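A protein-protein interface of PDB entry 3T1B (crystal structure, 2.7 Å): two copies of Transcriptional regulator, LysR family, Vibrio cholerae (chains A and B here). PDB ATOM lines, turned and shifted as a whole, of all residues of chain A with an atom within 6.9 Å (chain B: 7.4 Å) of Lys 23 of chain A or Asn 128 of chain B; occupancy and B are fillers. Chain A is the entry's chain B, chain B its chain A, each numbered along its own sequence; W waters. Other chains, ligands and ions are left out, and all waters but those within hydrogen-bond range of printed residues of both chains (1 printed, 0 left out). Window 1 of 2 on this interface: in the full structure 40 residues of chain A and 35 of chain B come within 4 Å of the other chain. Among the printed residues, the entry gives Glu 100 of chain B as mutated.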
ATOM      1  N   TYR A  18       9.951  26.642  -4.212  1.00  0.00           N
ATOM      2  CA  TYR A  18       9.329  27.780  -4.879  1.00  0.00           C
ATOM      3  C   TYR A  18       9.275  27.587  -6.390  1.00  0.00           C
ATOM      4  O   TYR A  18       8.237  27.810  -7.015  1.00  0.00           O
ATOM      5  CB  TYR A  18      10.066  29.078  -4.533  1.00  0.00           C
ATOM      6  CG  TYR A  18       9.773  29.602  -3.142  1.00  0.00           C
ATOM      7  CD1 TYR A  18       8.584  29.286  -2.496  1.00  0.00           C
ATOM      8  CD2 TYR A  18      10.683  30.415  -2.477  1.00  0.00           C
ATOM      9  CE1 TYR A  18       8.310  29.765  -1.227  1.00  0.00           C
ATOM     10  CE2 TYR A  18      10.418  30.896  -1.206  1.00  0.00           C
ATOM     11  CZ  TYR A  18       9.231  30.568  -0.587  1.00  0.00           C
ATOM     12  OH  TYR A  18       8.963  31.048   0.674  1.00  0.00           O
ATOM     13  N   THR A  19      10.393  27.165  -6.970  1.00  0.00           N
ATOM     14  CA  THR A  19      10.476  26.956  -8.412  1.00  0.00           C
ATOM     15  C   THR A  19       9.527  25.853  -8.877  1.00  0.00           C
ATOM     16  O   THR A  19       8.832  26.004  -9.880  1.00  0.00           O
ATOM     17  CB  THR A  19      11.908  26.608  -8.848  1.00  0.00           C
ATOM     18  OG1 THR A  19      12.373  25.483  -8.094  1.00  0.00           O
ATOM     19  CG2 THR A  19      12.833  27.791  -8.610  1.00  0.00           C
ATOM     20  N   SER A  20       9.502  24.744  -8.144  1.00  0.00           N
ATOM     21  CA  SER A  20       8.584  23.655  -8.456  1.00  0.00           C
ATOM     22  C   SER A  20       7.133  24.126  -8.418  1.00  0.00           C
ATOM     23  O   SER A  20       6.331  23.758  -9.276  1.00  0.00           O
ATOM     24  CB  SER A  20       8.778  22.486  -7.491  1.00  0.00           C
ATOM     25  OG  SER A  20      10.015  21.839  -7.720  1.00  0.00           O
ATOM     26  N   THR A  21       6.802  24.933  -7.415  1.00  0.00           N
ATOM     27  CA  THR A  21       5.454  25.475  -7.277  1.00  0.00           C
ATOM     28  C   THR A  21       5.134  26.431  -8.419  1.00  0.00           C
ATOM     29  O   THR A  21       4.017  26.446  -8.939  1.00  0.00           O
ATOM     30  CB  THR A  21       5.277  26.218  -5.937  1.00  0.00           C
ATOM     31  OG1 THR A  21       5.633  25.348  -4.857  1.00  0.00           O
ATOM     32  CG2 THR A  21       3.832  26.671  -5.764  1.00  0.00           C
ATOM     33  N   SER A  22       6.122  27.230  -8.807  1.00  0.00           N
ATOM     34  CA  SER A  22       5.957  28.166  -9.910  1.00  0.00           C
ATOM     35  C   SER A  22       5.634  27.426 -11.204  1.00  0.00           C
ATOM     36  O   SER A  22       4.771  27.845 -11.977  1.00  0.00           O
ATOM     37  CB  SER A  22       7.224  29.006 -10.091  1.00  0.00           C
ATOM     38  OG  SER A  22       7.061  29.962 -11.123  1.00  0.00           O
ATOM     39  N   LYS A  23       6.331  26.317 -11.428  1.00  0.00           N
ATOM     40  CA  LYS A  23       6.158  25.539 -12.648  1.00  0.00           C
ATOM     41  C   LYS A  23       4.797  24.854 -12.710  1.00  0.00           C
ATOM     42  O   LYS A  23       4.206  24.736 -13.782  1.00  0.00           O
ATOM     43  CB  LYS A  23       7.276  24.504 -12.787  1.00  0.00           C
ATOM     44  CG  LYS A  23       8.666  25.111 -12.909  1.00  0.00           C
ATOM     45  CD  LYS A  23       9.720  24.062 -13.245  1.00  0.00           C
ATOM     46  CE  LYS A  23       9.444  23.407 -14.592  1.00  0.00           C
ATOM     47  NZ  LYS A  23      10.543  22.485 -15.004  1.00  0.00           N
ATOM     48  N   LYS A  24       4.301  24.410 -11.561  1.00  0.00           N
ATOM     49  CA  LYS A  24       3.031  23.691 -11.503  1.00  0.00           C
ATOM     50  C   LYS A  24       1.813  24.614 -11.446  1.00  0.00           C
ATOM     51  O   LYS A  24       0.769  24.314 -12.026  1.00  0.00           O
ATOM     52  CB  LYS A  24       3.019  22.725 -10.319  1.00  0.00           C
ATOM     53  CG  LYS A  24       1.646  22.158  -9.997  1.00  0.00           C
ATOM     54  CD  LYS A  24       1.726  20.685  -9.616  1.00  0.00           C
ATOM     55  CE  LYS A  24       2.085  19.825 -10.824  1.00  0.00           C
ATOM     56  NZ  LYS A  24       1.930  18.370 -10.544  1.00  0.00           N
ATOM     57  N   THR A  25       1.949  25.736 -10.747  1.00  0.00           N
ATOM     58  CA  THR A  25       0.840  26.669 -10.595  1.00  0.00           C
ATOM     59  C   THR A  25       0.888  27.773 -11.646  1.00  0.00           C
ATOM     60  O   THR A  25      -0.095  28.479 -11.864  1.00  0.00           O
ATOM     61  CB  THR A  25       0.820  27.304  -9.189  1.00  0.00           C
ATOM     62  OG1 THR A  25       1.984  28.119  -9.009  1.00  0.00           O
ATOM     63  CG2 THR A  25       0.798  26.224  -8.119  1.00  0.00           C
ATOM     64  N   MET A  26       2.040  27.912 -12.294  1.00  0.00           N
ATOM     65  CA  MET A  26       2.241  28.940 -13.310  1.00  0.00           C
ATOM     66  C   MET A  26       2.231  30.338 -12.696  1.00  0.00           C
ATOM     67  O   MET A  26       1.996  31.333 -13.382  1.00  0.00           O
ATOM     68  CB  MET A  26       1.191  28.826 -14.416  1.00  0.00           C
ATOM     69  CG  MET A  26       1.756  29.041 -15.809  1.00  0.00           C
ATOM     70  SD  MET A  26       3.087  27.884 -16.193  1.00  0.00           S
ATOM     71  CE  MET A  26       2.231  26.317 -16.067  1.00  0.00           C
ATOM     72  N   ILE A  27       2.487  30.394 -11.394  1.00  0.00           N
ATOM     73  CA  ILE A  27       2.630  31.655 -10.680  1.00  0.00           C
ATOM     74  C   ILE A  27       4.110  32.010 -10.571  1.00  0.00           C
ATOM     75  O   ILE A  27       4.928  31.154 -10.234  1.00  0.00           O
ATOM     76  CB  ILE A  27       2.041  31.559  -9.264  1.00  0.00           C
ATOM     77  CG1 ILE A  27       0.561  31.180  -9.321  1.00  0.00           C
ATOM     78  CG2 ILE A  27       2.224  32.867  -8.517  1.00  0.00           C
ATOM     79  CD1 ILE A  27      -0.070  30.976  -7.959  1.00  0.00           C
ATOM     80  N   VAL A  29       7.709  33.092  -9.333  1.00  0.00           N
ATOM     81  CA  VAL A  29       8.381  32.870  -8.059  1.00  0.00           C
ATOM     82  C   VAL A  29       8.355  34.134  -7.205  1.00  0.00           C
ATOM     83  O   VAL A  29       8.178  34.070  -5.988  1.00  0.00           O
ATOM     84  CB  VAL A  29       9.845  32.426  -8.258  1.00  0.00           C
ATOM     85  CG1 VAL A  29      10.589  32.442  -6.935  1.00  0.00           C
ATOM     86  CG2 VAL A  29       9.899  31.044  -8.888  1.00  0.00           C
ATOM     87  N   ILE A  32       5.119  34.302  -5.352  1.00  0.00           N
ATOM     88  CA  ILE A  32       5.089  33.318  -4.278  1.00  0.00           C
ATOM     89  C   ILE A  32       5.937  33.796  -3.104  1.00  0.00           C
ATOM     90  O   ILE A  32       5.473  33.828  -1.965  1.00  0.00           O
ATOM     91  CB  ILE A  32       5.616  31.953  -4.753  1.00  0.00           C
ATOM     92  CG1 ILE A  32       4.798  31.452  -5.946  1.00  0.00           C
ATOM     93  CG2 ILE A  32       5.593  30.948  -3.613  1.00  0.00           C
ATOM     94  CD1 ILE A  32       5.336  30.178  -6.557  1.00  0.00           C
ATOM     95  N   ARG A  94      -6.113  23.000 -18.113  1.00  0.00           N
ATOM     96  CA  ARG A  94      -4.802  22.584 -17.639  1.00  0.00           C
ATOM     97  C   ARG A  94      -4.395  21.261 -18.281  1.00  0.00           C
ATOM     98  O   ARG A  94      -5.026  20.227 -18.054  1.00  0.00           O
ATOM     99  CB  ARG A  94      -4.794  22.480 -16.113  1.00  0.00           C
ATOM    100  CG  ARG A  94      -3.408  22.442 -15.505  1.00  0.00           C
ATOM    101  CD  ARG A  94      -3.454  22.852 -14.049  1.00  0.00           C
ATOM    102  NE  ARG A  94      -2.167  22.671 -13.389  1.00  0.00           N
ATOM    103  CZ  ARG A  94      -1.774  21.532 -12.830  1.00  0.00           C
ATOM    104  NH1 ARG A  94      -2.572  20.473 -12.861  1.00  0.00           N
ATOM    105  NH2 ARG A  94      -0.586  21.451 -12.244  1.00  0.00           N
ATOM    106  N   LEU A 124      -0.047  24.741 -20.289  1.00  0.00           N
ATOM    107  CA  LEU A 124       0.603  23.509 -20.722  1.00  0.00           C
ATOM    108  C   LEU A 124       1.754  23.115 -19.800  1.00  0.00           C
ATOM    109  O   LEU A 124       2.728  23.851 -19.650  1.00  0.00           O
ATOM    110  CB  LEU A 124       1.105  23.628 -22.163  1.00  0.00           C
ATOM    111  CG  LEU A 124       1.754  22.364 -22.734  1.00  0.00           C
ATOM    112  CD1 LEU A 124       0.744  21.226 -22.795  1.00  0.00           C
ATOM    113  CD2 LEU A 124       2.363  22.616 -24.103  1.00  0.00           C
ATOM    114  N   MET A 125       1.631  21.943 -19.186  1.00  0.00           N
ATOM    115  CA  MET A 125       2.667  21.419 -18.308  1.00  0.00           C
ATOM    116  C   MET A 125       3.330  20.211 -18.953  1.00  0.00           C
ATOM    117  O   MET A 125       2.701  19.164 -19.121  1.00  0.00           O
ATOM    118  CB  MET A 125       2.067  21.027 -16.960  1.00  0.00           C
ATOM    119  CG  MET A 125       3.010  20.276 -16.030  1.00  0.00           C
ATOM    120  SD  MET A 125       4.088  21.350 -15.063  1.00  0.00           S
ATOM    121  CE  MET A 125       4.436  20.298 -13.656  1.00  0.00           C
ATOM    122  N   MET A 126       4.602  20.360 -19.310  1.00  0.00           N
ATOM    123  CA  MET A 126       5.345  19.292 -19.971  1.00  0.00           C
ATOM    124  C   MET A 126       6.386  18.663 -19.048  1.00  0.00           C
ATOM    125  O   MET A 126       7.285  19.343 -18.558  1.00  0.00           O
ATOM    126  CB  MET A 126       6.023  19.833 -21.231  1.00  0.00           C
ATOM    127  CG  MET A 126       5.060  20.455 -22.226  1.00  0.00           C
ATOM    128  SD  MET A 126       5.875  21.551 -23.405  1.00  0.00           S
ATOM    129  CE  MET A 126       7.053  20.434 -24.156  1.00  0.00           C
ATOM    130  N   TRP A 138      -5.507  17.532 -13.390  1.00  0.00           N
ATOM    131  CA  TRP A 138      -5.449  17.840 -14.814  1.00  0.00           C
ATOM    132  C   TRP A 138      -6.808  17.753 -15.495  1.00  0.00           C
ATOM    133  O   TRP A 138      -7.673  16.974 -15.092  1.00  0.00           O
ATOM    134  CB  TRP A 138      -4.468  16.904 -15.521  1.00  0.00           C
ATOM    135  CG  TRP A 138      -3.104  16.916 -14.922  1.00  0.00           C
ATOM    136  CD1 TRP A 138      -2.545  15.951 -14.135  1.00  0.00           C
ATOM    137  CD2 TRP A 138      -2.121  17.945 -15.050  1.00  0.00           C
ATOM    138  NE1 TRP A 138      -1.272  16.315 -13.769  1.00  0.00           N
ATOM    139  CE2 TRP A 138      -0.987  17.540 -14.319  1.00  0.00           C
ATOM    140  CE3 TRP A 138      -2.085  19.176 -15.716  1.00  0.00           C
ATOM    141  CZ2 TRP A 138       0.163  18.313 -14.231  1.00  0.00           C
ATOM    142  CZ3 TRP A 138      -0.942  19.944 -15.629  1.00  0.00           C
ATOM    143  CH2 TRP A 138       0.164  19.510 -14.891  1.00  0.00           C
ATOM    144  N   ALA B  97      22.795  20.644 -17.965  1.00  0.00           N
ATOM    145  CA  ALA B  97      22.653  21.881 -18.724  1.00  0.00           C
ATOM    146  C   ALA B  97      21.205  22.378 -18.725  1.00  0.00           C
ATOM    147  O   ALA B  97      20.286  21.614 -18.434  1.00  0.00           O
ATOM    148  CB  ALA B  97      23.153  21.679 -20.147  1.00  0.00           C
ATOM    149  N   PRO B  98      21.000  23.667 -19.049  1.00  0.00           N
ATOM    150  CA  PRO B  98      19.667  24.286 -19.055  1.00  0.00           C
ATOM    151  C   PRO B  98      18.756  23.702 -20.132  1.00  0.00           C
ATOM    152  O   PRO B  98      19.227  23.353 -21.215  1.00  0.00           O
ATOM    153  CB  PRO B  98      19.966  25.759 -19.358  1.00  0.00           C
ATOM    154  CG  PRO B  98      21.397  25.948 -18.973  1.00  0.00           C
ATOM    155  CD  PRO B  98      22.056  24.655 -19.324  1.00  0.00           C
ATOM    156  N   SER B  99      17.464  23.613 -19.831  1.00  0.00           N
ATOM    157  CA  SER B  99      16.496  22.977 -20.722  1.00  0.00           C
ATOM    158  C   SER B  99      16.487  23.554 -22.138  1.00  0.00           C
ATOM    159  O   SER B  99      16.730  22.839 -23.109  1.00  0.00           O
ATOM    160  CB  SER B  99      15.086  23.064 -20.127  1.00  0.00           C
ATOM    161  OG  SER B  99      14.986  22.308 -18.929  1.00  0.00           O
ATOM    162  N   GLU B 100      16.205  24.848 -22.249  1.00  0.00           N
ATOM    163  CA  GLU B 100      15.943  25.468 -23.546  1.00  0.00           C
ATOM    164  C   GLU B 100      17.197  25.904 -24.305  1.00  0.00           C
ATOM    165  O   GLU B 100      17.204  25.926 -25.536  1.00  0.00           O
ATOM    166  CB  GLU B 100      15.020  26.674 -23.371  1.00  0.00           C
ATOM    167  CG  GLU B 100      13.907  26.464 -22.362  1.00  0.00           C
ATOM    168  CD  GLU B 100      12.941  25.370 -22.770  1.00  0.00           C
ATOM    169  OE1 GLU B 100      12.456  25.397 -23.921  1.00  0.00           O
ATOM    170  OE2 GLU B 100      12.662  24.483 -21.936  1.00  0.00           O
ATOM    171  N   MET B 126      19.108  17.666 -18.853  1.00  0.00           N
ATOM    172  CA  MET B 126      18.616  19.045 -18.872  1.00  0.00           C
ATOM    173  C   MET B 126      17.536  19.289 -17.816  1.00  0.00           C
ATOM    174  O   MET B 126      16.666  18.447 -17.601  1.00  0.00           O
ATOM    175  CB  MET B 126      18.081  19.413 -20.259  1.00  0.00           C
ATOM    176  CG  MET B 126      19.073  20.157 -21.142  1.00  0.00           C
ATOM    177  SD  MET B 126      19.911  19.101 -22.337  1.00  0.00           S
ATOM    178  CE  MET B 126      18.520  18.528 -23.307  1.00  0.00           C
ATOM    179  N   SER B 127      17.597  20.448 -17.164  1.00  0.00           N
ATOM    180  CA  SER B 127      16.626  20.802 -16.133  1.00  0.00           C
ATOM    181  C   SER B 127      16.369  22.307 -16.096  1.00  0.00           C
ATOM    182  O   SER B 127      17.188  23.095 -16.570  1.00  0.00           O
ATOM    183  CB  SER B 127      17.091  20.308 -14.758  1.00  0.00           C
ATOM    184  OG  SER B 127      18.385  20.789 -14.440  1.00  0.00           O
ATOM    185  N   ASN B 128      15.226  22.690 -15.535  1.00  0.00           N
ATOM    186  CA  ASN B 128      14.852  24.096 -15.396  1.00  0.00           C
ATOM    187  C   ASN B 128      15.333  24.711 -14.087  1.00  0.00           C
ATOM    188  O   ASN B 128      15.604  25.909 -14.014  1.00  0.00           O
ATOM    189  CB  ASN B 128      13.332  24.257 -15.505  1.00  0.00           C
ATOM    190  CG  ASN B 128      12.885  24.625 -16.904  1.00  0.00           C
ATOM    191  OD1 ASN B 128      13.684  25.083 -17.720  1.00  0.00           O
ATOM    192  ND2 ASN B 128      11.599  24.434 -17.188  1.00  0.00           N
ATOM    193  N   GLN B 129      15.437  23.881 -13.056  1.00  0.00           N
ATOM    194  CA  GLN B 129      15.760  24.355 -11.718  1.00  0.00           C
ATOM    195  C   GLN B 129      17.182  23.974 -11.321  1.00  0.00           C
ATOM    196  O   GLN B 129      17.427  22.869 -10.832  1.00  0.00           O
ATOM    197  CB  GLN B 129      14.749  23.795 -10.717  1.00  0.00           C
ATOM    198  CG  GLN B 129      13.308  24.138 -11.069  1.00  0.00           C
ATOM    199  CD  GLN B 129      12.326  23.066 -10.646  1.00  0.00           C
ATOM    200  OE1 GLN B 129      11.950  22.206 -11.442  1.00  0.00           O
ATOM    201  NE2 GLN B 129      11.898  23.116  -9.392  1.00  0.00           N
ATOM    202  N   ALA B 130      18.115  24.897 -11.531  1.00  0.00           N
ATOM    203  CA  ALA B 130      19.530  24.650 -11.269  1.00  0.00           C
ATOM    204  C   ALA B 130      19.856  24.607  -9.777  1.00  0.00           C
ATOM    205  O   ALA B 130      20.918  24.130  -9.381  1.00  0.00           O
ATOM    206  CB  ALA B 130      20.389  25.697 -11.971  1.00  0.00           C
ATOM    207  N   ASP B 131      18.945  25.109  -8.952  1.00  0.00           N
ATOM    208  CA  ASP B 131      19.150  25.103  -7.508  1.00  0.00           C
ATOM    209  C   ASP B 131      18.700  23.783  -6.888  1.00  0.00           C
ATOM    210  O   ASP B 131      19.209  23.369  -5.845  1.00  0.00           O
ATOM    211  CB  ASP B 131      18.412  26.276  -6.856  1.00  0.00           C
ATOM    212  CG  ASP B 131      19.181  27.583  -6.961  1.00  0.00           C
ATOM    213  OD1 ASP B 131      20.176  27.634  -7.715  1.00  0.00           O
ATOM    214  OD2 ASP B 131      18.789  28.560  -6.287  1.00  0.00           O
ATOM    215  N   ASP B 132      17.751  23.123  -7.545  1.00  0.00           N
ATOM    216  CA  ASP B 132      17.164  21.892  -7.022  1.00  0.00           C
ATOM    217  C   ASP B 132      18.039  20.658  -7.224  1.00  0.00           C
ATOM    218  O   ASP B 132      17.669  19.559  -6.809  1.00  0.00           O
ATOM    219  CB  ASP B 132      15.781  21.651  -7.637  1.00  0.00           C
ATOM    220  CG  ASP B 132      14.684  22.419  -6.928  1.00  0.00           C
ATOM    221  OD1 ASP B 132      14.961  23.527  -6.425  1.00  0.00           O
ATOM    222  OD2 ASP B 132      13.543  21.912  -6.869  1.00  0.00           O
ATOM    223  N   ARG B 143      24.471  26.362 -16.055  1.00  0.00           N
ATOM    224  CA  ARG B 143      23.225  26.911 -15.535  1.00  0.00           C
ATOM    225  C   ARG B 143      23.087  28.410 -15.783  1.00  0.00           C
ATOM    226  O   ARG B 143      24.075  29.106 -16.020  1.00  0.00           O
ATOM    227  CB  ARG B 143      23.119  26.635 -14.036  1.00  0.00           C
ATOM    228  CG  ARG B 143      24.233  27.264 -13.216  1.00  0.00           C
ATOM    229  CD  ARG B 143      23.847  27.352 -11.753  1.00  0.00           C
ATOM    230  NE  ARG B 143      22.692  28.219 -11.555  1.00  0.00           N
ATOM    231  CZ  ARG B 143      22.030  28.330 -10.409  1.00  0.00           C
ATOM    232  NH1 ARG B 143      22.404  27.619  -9.356  1.00  0.00           N
ATOM    233  NH2 ARG B 143      20.990  29.148 -10.317  1.00  0.00           N
ATOM    234  N   VAL B 144      21.852  28.894 -15.723  1.00  0.00           N
ATOM    235  CA  VAL B 144      21.578  30.320 -15.813  1.00  0.00           C
ATOM    236  C   VAL B 144      21.624  30.933 -14.420  1.00  0.00           C
ATOM    237  O   VAL B 144      21.096  30.362 -13.467  1.00  0.00           O
ATOM    238  CB  VAL B 144      20.193  30.583 -16.428  1.00  0.00           C
ATOM    239  CG1 VAL B 144      19.865  32.071 -16.395  1.00  0.00           C
ATOM    240  CG2 VAL B 144      20.139  30.043 -17.845  1.00  0.00           C
ATOM    241  N   TYR B 192       7.687  29.511 -18.322  1.00  0.00           N
ATOM    242  CA  TYR B 192       8.688  29.466 -17.264  1.00  0.00           C
ATOM    243  C   TYR B 192      10.069  29.433 -17.907  1.00  0.00           C
ATOM    244  O   TYR B 192      10.260  28.775 -18.932  1.00  0.00           O
ATOM    245  CB  TYR B 192       8.468  28.228 -16.388  1.00  0.00           C
ATOM    246  CG  TYR B 192       9.299  28.194 -15.124  1.00  0.00           C
ATOM    247  CD1 TYR B 192       8.838  28.769 -13.948  1.00  0.00           C
ATOM    248  CD2 TYR B 192      10.544  27.584 -15.108  1.00  0.00           C
ATOM    249  CE1 TYR B 192       9.597  28.741 -12.793  1.00  0.00           C
ATOM    250  CE2 TYR B 192      11.311  27.548 -13.960  1.00  0.00           C
ATOM    251  CZ  TYR B 192      10.835  28.127 -12.805  1.00  0.00           C
ATOM    252  OH  TYR B 192      11.599  28.092 -11.659  1.00  0.00           O
ATOM    253  N   PRO B 193      11.045  30.135 -17.311  1.00  0.00           N
ATOM    254  CA  PRO B 193      10.948  30.900 -16.062  1.00  0.00           C
ATOM    255  C   PRO B 193      10.496  32.348 -16.267  1.00  0.00           C
ATOM    256  O   PRO B 193      10.418  33.107 -15.299  1.00  0.00           O
ATOM    257  CB  PRO B 193      12.387  30.877 -15.551  1.00  0.00           C
ATOM    258  CG  PRO B 193      13.202  30.893 -16.801  1.00  0.00           C
ATOM    259  CD  PRO B 193      12.427  30.097 -17.821  1.00  0.00           C
ATOM    260  N   LEU B 195       7.865  34.385 -16.383  1.00  0.00           N
ATOM    261  CA  LEU B 195       6.452  34.595 -16.087  1.00  0.00           C
ATOM    262  C   LEU B 195       6.186  36.039 -15.672  1.00  0.00           C
ATOM    263  O   LEU B 195       5.276  36.689 -16.189  1.00  0.00           O
ATOM    264  CB  LEU B 195       5.978  33.632 -15.000  1.00  0.00           C
ATOM    265  CG  LEU B 195       6.134  32.148 -15.334  1.00  0.00           C
ATOM    266  CD1 LEU B 195       5.475  31.280 -14.274  1.00  0.00           C
ATOM    267  CD2 LEU B 195       5.555  31.851 -16.709  1.00  0.00           C
ATOM    268  N   ALA B 217       3.092  27.972 -20.489  1.00  0.00           N
ATOM    269  CA  ALA B 217       3.707  26.648 -20.524  1.00  0.00           C
ATOM    270  C   ALA B 217       4.885  26.507 -19.559  1.00  0.00           C
ATOM    271  O   ALA B 217       5.393  27.494 -19.026  1.00  0.00           O
ATOM    272  CB  ALA B 217       4.133  26.300 -21.945  1.00  0.00           C
ATOM    273  N   SER B 218       5.312  25.267 -19.346  1.00  0.00           N
ATOM    274  CA  SER B 218       6.404  24.972 -18.425  1.00  0.00           C
ATOM    275  C   SER B 218       7.762  25.104 -19.105  1.00  0.00           C
ATOM    276  O   SER B 218       8.803  24.968 -18.463  1.00  0.00           O
ATOM    277  CB  SER B 218       6.246  23.568 -17.838  1.00  0.00           C
ATOM    278  OG  SER B 218       6.157  22.603 -18.872  1.00  0.00           O
ATOM    279  N   ALA B 219       7.743  25.365 -20.408  1.00  0.00           N
ATOM    280  CA  ALA B 219       8.965  25.557 -21.182  1.00  0.00           C
ATOM    281  C   ALA B 219       8.733  26.606 -22.266  1.00  0.00           C
ATOM    282  O   ALA B 219       7.611  26.776 -22.742  1.00  0.00           O
ATOM    283  CB  ALA B 219       9.420  24.244 -21.796  1.00  0.00           C
ATOM    284  N   LEU B 220       9.797  27.298 -22.659  1.00  0.00           N
ATOM    285  CA  LEU B 220       9.680  28.432 -23.575  1.00  0.00           C
ATOM    286  C   LEU B 220       9.507  28.049 -25.047  1.00  0.00           C
ATOM    287  O   LEU B 220       8.945  28.816 -25.829  1.00  0.00           O
ATOM    288  CB  LEU B 220      10.871  29.381 -23.412  1.00  0.00           C
ATOM    289  CG  LEU B 220      10.825  30.282 -22.177  1.00  0.00           C
ATOM    290  CD1 LEU B 220      12.104  31.088 -22.053  1.00  0.00           C
ATOM    291  CD2 LEU B 220       9.612  31.198 -22.233  1.00  0.00           C
HETATM  292  O   HOH W   1      15.286  25.951  -8.098  1.00  0.00           O
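The side-chain hydroxyl (OG) of Ser 20 of chain A lies within hydrogen-bond range of the side-chain amide nitrogen (NE2) of Gln 129 of chain B. The side-chain amino group (NZ) of Lys 23 of chain A lies close to the side-chain amide nitrogen (ND2) of Asn 128 of chain B (3.1 Å). The side-chain amide nitrogen of Gln 129 of chain B sits at hydrogen-bond distance from the side-chain hydroxyl of Thr 19 of chain A (2.7 Å). The side-chain sulfur (SD) of Met 26 of chain A sits close to the backbone carbonyl oxygen (O) of Ala 217 of chain B, 3.7 Å away. The backbone NH (N) of Ser 218 of chain B is in hydrogen-bond range of the backbone carbonyl oxygen (O) of Leu 124 of chain A. OG of Ser 218 of chain B lies within hydrogen-bond range of N of Met 126 of chain A (2.8 Å).
O of Ile 27 of chain A is in hydrogen-bond range of OG of Ser 22 of chain A (2.6 Å). The side-chain amide nitrogen (NE2) of Gln 129 of chain B is in hydrogen-bond range of the side-chain carboxylate (OD2) of Asp 132 of chain B (3.2 Å). The side-chain amide nitrogen of Asn 128 of chain B lies within hydrogen-bond range of the backbone carbonyl oxygen of Ser 218 of chain B. The side-chain amide oxygen of Asn 128 of chain B lies within hydrogen-bond range of the side-chain hydroxyl of Ser 99 of chain B (3.3 Å). The backbone NH (N) of Tyr 192 of chain B sits at hydrogen-bond distance from the backbone carbonyl oxygen (O) of Ala 217 of chain B, at 3.1 Å.
Among the printed residues, pairs that only touch across the chains: Leu 124 of chain A with Ala 217 of chain B (3.1 Å), Thr 19 of chain A with Tyr 192 of chain B (3.2 Å), Ser 22 of chain A with Tyr 192 of chain B (3.3 Å), Lys 23 of chain A with Gln 129 of chain B (3.4 Å), Met 26 of chain A with Leu 195 of chain B (3.6 Å), Ser 20 of chain A with Asp 132 of chain B (3.6 Å), Thr 19 of chain A with Asp 132 of chain B (3.6 Å), Met 125 of chain A with Ser 218 of chain B (3.7 Å), Lys 23 of chain A with Tyr 192 of chain B (3.7 Å) and Ser 22 of chain A with Leu 195 of chain B (3.8 Å).
Printed residues of chain B within 4 Å of Ser 20 of chain A: Gln 129 and Asp 132. Of chain B, only Asn 128 (3.1 Å), Gln 129 (3.4 Å) and Tyr 192 (3.7 Å) come within 4 Å of Lys 23 of chain A. Trp 138 of chain A touches none of the printed residues of chain B. Ser 99 of chain B touches none of the printed residues of chain A. Asn 128 of chain B touches just one residue of chain A: Lys 23. Printed residues of chain A within 4 Å of Gln 129 of chain B: Thr 19 (2.7 Å), Ser 20 (2.8 Å) and Lys 23 (3.4 Å). Of the printed residues of chain A, Tyr 192 of chain B touches Thr 19 (3.2 Å), Ser 22 (3.3 Å) and Lys 23 (3.7 Å). Of the printed residues of chain A, Ser 218 of chain B touches Leu 124, Met 125 and Met 126. The nearest residue of chain B that does not touch Lys 23 of chain A is Ser 218 of chain B (4.2 Å). The nearest residue of chain A that does not touch Asn 128 of chain B is Thr 19 of chain A (6.4 Å).
Hydrophobic or aromatic side chains of chain A that line the printed part of chain B: Met 26 and Met 126. Among the printed residues, 16 pairs touch across the chains. Among the printed residues, no Asp or Glu carboxylate lies within 4 Å of a Lys or Arg side-chain nitrogen of the other chain.
1 position is printed for both chains.
Water W1 bridges the side-chain hydroxyl (OG1) of Thr 19 of chain A (3.0 Å) and the side-chain carboxylate (OD1) of Asp 132 of chain B (3.0 Å).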
